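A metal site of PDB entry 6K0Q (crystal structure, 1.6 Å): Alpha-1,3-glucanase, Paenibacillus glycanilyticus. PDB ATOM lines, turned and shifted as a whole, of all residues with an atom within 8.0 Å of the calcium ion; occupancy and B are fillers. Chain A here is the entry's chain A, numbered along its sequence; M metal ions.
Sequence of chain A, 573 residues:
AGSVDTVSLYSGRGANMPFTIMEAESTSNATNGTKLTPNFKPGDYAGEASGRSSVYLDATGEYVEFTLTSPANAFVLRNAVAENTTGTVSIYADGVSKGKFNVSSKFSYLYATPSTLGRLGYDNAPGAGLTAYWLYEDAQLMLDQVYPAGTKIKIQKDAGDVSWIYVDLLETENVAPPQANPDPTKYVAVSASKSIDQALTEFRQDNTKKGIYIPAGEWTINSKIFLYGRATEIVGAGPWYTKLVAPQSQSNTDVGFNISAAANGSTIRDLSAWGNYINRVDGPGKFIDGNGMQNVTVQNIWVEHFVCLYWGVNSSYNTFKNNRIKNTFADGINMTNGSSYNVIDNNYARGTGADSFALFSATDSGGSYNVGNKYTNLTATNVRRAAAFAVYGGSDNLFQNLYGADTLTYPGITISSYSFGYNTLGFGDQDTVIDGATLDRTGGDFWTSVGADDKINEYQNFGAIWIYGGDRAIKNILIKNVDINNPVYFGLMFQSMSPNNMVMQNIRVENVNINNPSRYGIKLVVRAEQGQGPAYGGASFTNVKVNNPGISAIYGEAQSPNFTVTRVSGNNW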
ATOM      1  N   ILE A  21      12.434  24.692  21.383  1.00  0.00           N
ATOM      2  CA  ILE A  21      11.711  23.540  20.864  1.00  0.00           C
ATOM      3  C   ILE A  21      11.529  22.541  22.009  1.00  0.00           C
ATOM      4  O   ILE A  21      12.497  22.161  22.667  1.00  0.00           O
ATOM      5  CB  ILE A  21      12.453  22.887  19.701  1.00  0.00           C
ATOM      6  CG1 ILE A  21      12.536  23.858  18.525  1.00  0.00           C
ATOM      7  CG2 ILE A  21      11.773  21.569  19.311  1.00  0.00           C
ATOM      8  CD1 ILE A  21      13.225  23.271  17.323  1.00  0.00           C
ATOM      9  N   MET A  22      10.283  22.113  22.220  1.00  0.00           N
ATOM     10  CA  MET A  22       9.966  21.120  23.226  1.00  0.00           C
ATOM     11  C   MET A  22       9.207  19.972  22.570  1.00  0.00           C
ATOM     12  O   MET A  22       8.175  20.208  21.914  1.00  0.00           O
ATOM     13  CB  MET A  22       9.110  21.696  24.353  1.00  0.00           C
ATOM     14  CG  MET A  22       9.717  22.894  25.015  1.00  0.00           C
ATOM     15  SD  MET A  22       8.458  23.681  25.992  1.00  0.00           S
ATOM     16  CE  MET A  22       9.476  24.798  26.943  1.00  0.00           C
ATOM     17  N   GLU A  23       9.707  18.761  22.749  1.00  0.00           N
ATOM     18  CA  GLU A  23       9.031  17.583  22.220  1.00  0.00           C
ATOM     19  C   GLU A  23       7.766  17.302  23.018  1.00  0.00           C
ATOM     20  O   GLU A  23       7.781  17.347  24.253  1.00  0.00           O
ATOM     21  CB  GLU A  23       9.954  16.370  22.272  1.00  0.00           C
ATOM     22  CG  GLU A  23      11.225  16.529  21.451  1.00  0.00           C
ATOM     23  CD  GLU A  23      10.965  16.443  19.943  1.00  0.00           C
ATOM     24  OE1 GLU A  23       9.817  16.161  19.498  1.00  0.00           O
ATOM     25  OE2 GLU A  23      11.943  16.629  19.187  1.00  0.00           O
ATOM     26  N   ALA A  24       6.671  17.012  22.311  1.00  0.00           N
ATOM     27  CA  ALA A  24       5.417  16.739  22.993  1.00  0.00           C
ATOM     28  C   ALA A  24       5.554  15.568  23.951  1.00  0.00           C
ATOM     29  O   ALA A  24       5.010  15.581  25.067  1.00  0.00           O
ATOM     30  CB  ALA A  24       4.305  16.480  21.969  1.00  0.00           C
ATOM     31  N   GLU A  25       6.314  14.554  23.543  1.00  0.00           N
ATOM     32  CA  GLU A  25       6.459  13.300  24.268  1.00  0.00           C
ATOM     33  C   GLU A  25       7.449  13.383  25.413  1.00  0.00           C
ATOM     34  O   GLU A  25       7.702  12.368  26.062  1.00  0.00           O
ATOM     35  CB  GLU A  25       6.888  12.183  23.300  1.00  0.00           C
ATOM     36  CG  GLU A  25       8.294  12.357  22.693  1.00  0.00           C
ATOM     37  CD  GLU A  25       8.300  13.206  21.413  1.00  0.00           C
ATOM     38  OE1 GLU A  25       7.310  13.923  21.131  1.00  0.00           O
ATOM     39  OE2 GLU A  25       9.313  13.156  20.686  1.00  0.00           O
ATOM     40  N   SER A  26       8.004  14.565  25.678  1.00  0.00           N
ATOM     41  CA  SER A  26       8.991  14.679  26.743  1.00  0.00           C
ATOM     42  C   SER A  26       8.382  14.218  28.068  1.00  0.00           C
ATOM     43  O   SER A  26       7.194  14.418  28.322  1.00  0.00           O
ATOM     44  CB  SER A  26       9.482  16.120  26.854  1.00  0.00           C
ATOM     45  OG  SER A  26       9.927  16.444  28.166  1.00  0.00           O
ATOM     46  N   TYR A  45       3.532   7.694  11.679  1.00  0.00           N
ATOM     47  CA  TYR A  45       3.395   8.875  12.533  1.00  0.00           C
ATOM     48  C   TYR A  45       4.476   8.937  13.621  1.00  0.00           C
ATOM     49  O   TYR A  45       4.775  10.031  14.106  1.00  0.00           O
ATOM     50  CB  TYR A  45       1.989   8.953  13.158  1.00  0.00           C
ATOM     51  CG  TYR A  45       0.936   9.240  12.104  1.00  0.00           C
ATOM     52  CD1 TYR A  45       0.882  10.473  11.466  1.00  0.00           C
ATOM     53  CD2 TYR A  45       0.037   8.262  11.726  1.00  0.00           C
ATOM     54  CE1 TYR A  45      -0.075  10.719  10.480  1.00  0.00           C
ATOM     55  CE2 TYR A  45      -0.925   8.498  10.750  1.00  0.00           C
ATOM     56  CZ  TYR A  45      -0.965   9.730  10.129  1.00  0.00           C
ATOM     57  OH  TYR A  45      -1.918   9.965   9.157  1.00  0.00           O
ATOM     58  N   ALA A  46       5.061   7.807  13.999  1.00  0.00           N
ATOM     59  CA  ALA A  46       6.228   7.868  14.873  1.00  0.00           C
ATOM     60  C   ALA A  46       7.492   8.078  14.057  1.00  0.00           C
ATOM     61  O   ALA A  46       8.287   8.978  14.349  1.00  0.00           O
ATOM     62  CB  ALA A  46       6.342   6.588  15.707  1.00  0.00           C
ATOM     63  N   GLU A  48       8.151   9.493  11.356  1.00  0.00           N
ATOM     64  CA  GLU A  48       8.330  10.808  10.762  1.00  0.00           C
ATOM     65  C   GLU A  48       8.310  11.935  11.782  1.00  0.00           C
ATOM     66  O   GLU A  48       8.461  13.103  11.405  1.00  0.00           O
ATOM     67  CB  GLU A  48       7.280  11.055   9.691  1.00  0.00           C
ATOM     68  CG  GLU A  48       7.432  10.143   8.464  1.00  0.00           C
ATOM     69  CD  GLU A  48       6.709  10.670   7.237  1.00  0.00           C
ATOM     70  OE1 GLU A  48       6.144  11.789   7.320  1.00  0.00           O
ATOM     71  OE2 GLU A  48       6.716   9.988   6.195  1.00  0.00           O
ATOM     72  N   ALA A  49       8.124  11.622  13.047  1.00  0.00           N
ATOM     73  CA  ALA A  49       8.078  12.651  14.073  1.00  0.00           C
ATOM     74  C   ALA A  49       9.476  13.063  14.513  1.00  0.00           C
ATOM     75  O   ALA A  49      10.441  12.287  14.447  1.00  0.00           O
ATOM     76  CB  ALA A  49       7.291  12.161  15.297  1.00  0.00           C
ATOM     77  N   SER A  50       9.590  14.311  14.960  1.00  0.00           N
ATOM     78  CA  SER A  50      10.797  14.738  15.654  1.00  0.00           C
ATOM     79  C   SER A  50      10.960  13.878  16.902  1.00  0.00           C
ATOM     80  O   SER A  50      10.003  13.648  17.649  1.00  0.00           O
ATOM     81  CB  SER A  50      10.698  16.224  16.002  1.00  0.00           C
ATOM     82  OG  SER A  50      11.888  16.683  16.642  1.00  0.00           O
ATOM     83  N   GLY A  51      12.171  13.365  17.117  1.00  0.00           N
ATOM     84  CA  GLY A  51      12.387  12.426  18.206  1.00  0.00           C
ATOM     85  C   GLY A  51      11.782  11.049  17.974  1.00  0.00           C
ATOM     86  O   GLY A  51      11.801  10.215  18.892  1.00  0.00           O
ATOM     87  N   ARG A  52      11.261  10.806  16.776  1.00  0.00           N
ATOM     88  CA  ARG A  52      10.574   9.570  16.400  1.00  0.00           C
ATOM     89  C   ARG A  52       9.380   9.280  17.307  1.00  0.00           C
ATOM     90  O   ARG A  52       8.967   8.133  17.466  1.00  0.00           O
ATOM     91  CB  ARG A  52      11.532   8.371  16.356  1.00  0.00           C
ATOM     92  CG  ARG A  52      12.795   8.643  15.558  1.00  0.00           C
ATOM     93  CD  ARG A  52      12.513   8.882  14.064  1.00  0.00           C
ATOM     94  NE  ARG A  52      13.770   9.144  13.374  1.00  0.00           N
ATOM     95  CZ  ARG A  52      14.024   8.854  12.089  1.00  0.00           C
ATOM     96  NH1 ARG A  52      13.097   8.300  11.309  1.00  0.00           N
ATOM     97  NH2 ARG A  52      15.240   9.122  11.610  1.00  0.00           N
ATOM     98  N   SER A  53       8.774  10.326  17.870  1.00  0.00           N
ATOM     99  CA  SER A  53       7.561  10.069  18.636  1.00  0.00           C
ATOM    100  C   SER A  53       6.720  11.333  18.684  1.00  0.00           C
ATOM    101  O   SER A  53       7.210  12.460  18.473  1.00  0.00           O
ATOM    102  CB  SER A  53       7.906   9.529  20.033  1.00  0.00           C
ATOM    103  OG  SER A  53       6.789   9.542  20.902  1.00  0.00           O
ATOM    104  N   SER A  54       5.427  11.133  18.915  1.00  0.00           N
ATOM    105  CA  SER A  54       4.457  12.193  19.093  1.00  0.00           C
ATOM    106  C   SER A  54       3.471  11.747  20.159  1.00  0.00           C
ATOM    107  O   SER A  54       3.483  10.599  20.598  1.00  0.00           O
ATOM    108  CB  SER A  54       3.687  12.514  17.792  1.00  0.00           C
ATOM    109  OG  SER A  54       4.535  13.048  16.812  1.00  0.00           O
ATOM    110  N   VAL A  55       2.593  12.655  20.553  1.00  0.00           N
ATOM    111  CA  VAL A  55       1.475  12.295  21.422  1.00  0.00           C
ATOM    112  C   VAL A  55       0.201  12.440  20.619  1.00  0.00           C
ATOM    113  O   VAL A  55      -0.099  13.513  20.088  1.00  0.00           O
ATOM    114  CB  VAL A  55       1.433  13.134  22.703  1.00  0.00           C
ATOM    115  CG1 VAL A  55       0.263  12.650  23.556  1.00  0.00           C
ATOM    116  CG2 VAL A  55       2.741  13.015  23.487  1.00  0.00           C
ATOM    117  N   ARG A  78       4.041  21.558  15.482  1.00  0.00           N
ATOM    118  CA  ARG A  78       4.199  20.535  14.452  1.00  0.00           C
ATOM    119  C   ARG A  78       3.274  19.383  14.787  1.00  0.00           C
ATOM    120  O   ARG A  78       3.283  18.874  15.910  1.00  0.00           O
ATOM    121  CB  ARG A  78       5.658  20.040  14.350  1.00  0.00           C
ATOM    122  CG  ARG A  78       5.900  19.157  13.128  1.00  0.00           C
ATOM    123  CD  ARG A  78       7.362  18.772  12.999  1.00  0.00           C
ATOM    124  NE  ARG A  78       7.716  18.398  11.621  1.00  0.00           N
ATOM    125  CZ  ARG A  78       7.993  17.162  11.218  1.00  0.00           C
ATOM    126  NH1 ARG A  78       7.934  16.125  12.058  1.00  0.00           N
ATOM    127  NH2 ARG A  78       8.327  16.932   9.944  1.00  0.00           N
ATOM    128  N   TYR A 136       3.608  15.197   8.548  1.00  0.00           N
ATOM    129  CA  TYR A 136       3.536  16.289   9.503  1.00  0.00           C
ATOM    130  C   TYR A 136       3.523  17.647   8.809  1.00  0.00           C
ATOM    131  O   TYR A 136       4.039  17.809   7.702  1.00  0.00           O
ATOM    132  CB  TYR A 136       4.707  16.198  10.498  1.00  0.00           C
ATOM    133  CG  TYR A 136       4.444  15.128  11.533  1.00  0.00           C
ATOM    134  CD1 TYR A 136       3.710  15.417  12.679  1.00  0.00           C
ATOM    135  CD2 TYR A 136       4.861  13.805  11.331  1.00  0.00           C
ATOM    136  CE1 TYR A 136       3.420  14.440  13.630  1.00  0.00           C
ATOM    137  CE2 TYR A 136       4.593  12.815  12.303  1.00  0.00           C
ATOM    138  CZ  TYR A 136       3.859  13.145  13.435  1.00  0.00           C
ATOM    139  OH  TYR A 136       3.575  12.188  14.377  1.00  0.00           O
ATOM    140  N   VAL A 167       0.490  15.333  18.011  1.00  0.00           N
ATOM    141  CA  VAL A 167       1.252  16.510  18.425  1.00  0.00           C
ATOM    142  C   VAL A 167       2.711  16.087  18.560  1.00  0.00           C
ATOM    143  O   VAL A 167       3.048  15.253  19.411  1.00  0.00           O
ATOM    144  CB  VAL A 167       0.714  17.088  19.729  1.00  0.00           C
ATOM    145  CG1 VAL A 167       1.532  18.318  20.132  1.00  0.00           C
ATOM    146  CG2 VAL A 167      -0.767  17.434  19.599  1.00  0.00           C
ATOM    147  N   ASP A 168       3.583  16.669  17.731  1.00  0.00           N
ATOM    148  CA  ASP A 168       4.985  16.251  17.652  1.00  0.00           C
ATOM    149  C   ASP A 168       5.891  17.110  18.536  1.00  0.00           C
ATOM    150  O   ASP A 168       6.640  16.577  19.368  1.00  0.00           O
ATOM    151  CB  ASP A 168       5.421  16.280  16.177  1.00  0.00           C
ATOM    152  CG  ASP A 168       6.853  15.817  15.973  1.00  0.00           C
ATOM    153  OD1 ASP A 168       7.486  15.300  16.917  1.00  0.00           O
ATOM    154  OD2 ASP A 168       7.357  15.960  14.840  1.00  0.00           O
ATOM    155  N   LEU A 169       5.864  18.422  18.344  1.00  0.00           N
ATOM    156  CA  LEU A 169       6.688  19.341  19.109  1.00  0.00           C
ATOM    157  C   LEU A 169       5.996  20.698  19.121  1.00  0.00           C
ATOM    158  O   LEU A 169       5.085  20.959  18.331  1.00  0.00           O
ATOM    159  CB  LEU A 169       8.107  19.463  18.534  1.00  0.00           C
ATOM    160  CG  LEU A 169       8.282  19.958  17.077  1.00  0.00           C
ATOM    161  CD1 LEU A 169       8.149  21.495  16.911  1.00  0.00           C
ATOM    162  CD2 LEU A 169       9.634  19.524  16.549  1.00  0.00           C
ATOM    163  N   LEU A 170       6.504  21.576  19.987  1.00  0.00           N
ATOM    164  CA  LEU A 170       6.053  22.953  20.106  1.00  0.00           C
ATOM    165  C   LEU A 170       7.265  23.859  20.048  1.00  0.00           C
ATOM    166  O   LEU A 170       8.203  23.666  20.823  1.00  0.00           O
ATOM    167  CB  LEU A 170       5.302  23.155  21.436  1.00  0.00           C
ATOM    168  CG  LEU A 170       4.668  24.526  21.713  1.00  0.00           C
ATOM    169  CD1 LEU A 170       3.438  24.685  20.841  1.00  0.00           C
ATOM    170  CD2 LEU A 170       4.310  24.618  23.194  1.00  0.00           C
ATOM    171  N   ASN A 382      14.333  16.690  10.855  1.00  0.00           N
ATOM    172  CA  ASN A 382      13.183  16.185  10.115  1.00  0.00           C
ATOM    173  C   ASN A 382      13.406  16.320   8.603  1.00  0.00           C
ATOM    174  O   ASN A 382      12.602  16.911   7.885  1.00  0.00           O
ATOM    175  CB  ASN A 382      11.898  16.892  10.524  1.00  0.00           C
ATOM    176  CG  ASN A 382      11.446  16.512  11.915  1.00  0.00           C
ATOM    177  OD1 ASN A 382      11.351  17.375  12.786  1.00  0.00           O
ATOM    178  ND2 ASN A 382      11.166  15.228  12.132  1.00  0.00           N
ATOM    179  N   ASP A 406      16.963  13.085  12.703  1.00  0.00           N
ATOM    180  CA  ASP A 406      15.699  12.535  12.222  1.00  0.00           C
ATOM    181  C   ASP A 406      15.573  12.664  10.696  1.00  0.00           C
ATOM    182  O   ASP A 406      14.676  13.318  10.174  1.00  0.00           O
ATOM    183  CB  ASP A 406      14.524  13.170  12.950  1.00  0.00           C
ATOM    184  CG  ASP A 406      14.473  12.770  14.402  1.00  0.00           C
ATOM    185  OD1 ASP A 406      14.685  11.566  14.681  1.00  0.00           O
ATOM    186  OD2 ASP A 406      14.226  13.642  15.269  1.00  0.00           O
ATOM    187  N   ARG A 441      19.735  10.123  15.521  1.00  0.00           N
ATOM    188  CA  ARG A 441      18.788   9.300  14.760  1.00  0.00           C
ATOM    189  C   ARG A 441      18.853   9.617  13.254  1.00  0.00           C
ATOM    190  O   ARG A 441      17.820   9.843  12.598  1.00  0.00           O
ATOM    191  CB  ARG A 441      17.369   9.480  15.318  1.00  0.00           C
ATOM    192  CG  ARG A 441      17.238   9.112  16.808  1.00  0.00           C
ATOM    193  CD  ARG A 441      15.888   9.495  17.417  1.00  0.00           C
ATOM    194  NE  ARG A 441      15.631  10.917  17.247  1.00  0.00           N
ATOM    195  CZ  ARG A 441      16.087  11.872  18.053  1.00  0.00           C
ATOM    196  NH1 ARG A 441      16.791  11.558  19.137  1.00  0.00           N
ATOM    197  NH2 ARG A 441      15.830  13.142  17.771  1.00  0.00           N
HETATM  198 CA    CA M   1       8.218  14.574  18.940  1.00  0.00          CA
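The backbone NH (N) of Ser 50 sits close to the side-chain amide nitrogen (ND2) of Asn 382.
The backbone carbonyl oxygen (O) of Asp 168 sits close to the backbone NH (N) of Ala 24 (3.0 Å).
The side-chain carboxylate (OD2) of Asp 168 is in salt-bridge range of the guanidinium group (NH1) of Arg 78 (2.8 Å).
The nearest printed residue that does not touch the calcium ion is Ser 54 (4.4 Å).
OD1 of Asp 168 binds the calcium ion, 2.3 Å away.
OE1 of Glu 23 is bound to the calcium ion (2.3 Å).
The backbone carbonyl oxygen (O) of Ser 53 binds the calcium ion.
O of Ser 50 is bound to the calcium ion (2.4 Å).
The side-chain carboxylate (OE1) of Glu 25 binds the calcium ion, at 2.5 Å.
The calcium ion is bound by OE2 of Glu 25, 2.5 Å away.
The calcium ion is bound by the backbone carbonyl oxygen (O) of Asp 168 (2.6 Å).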
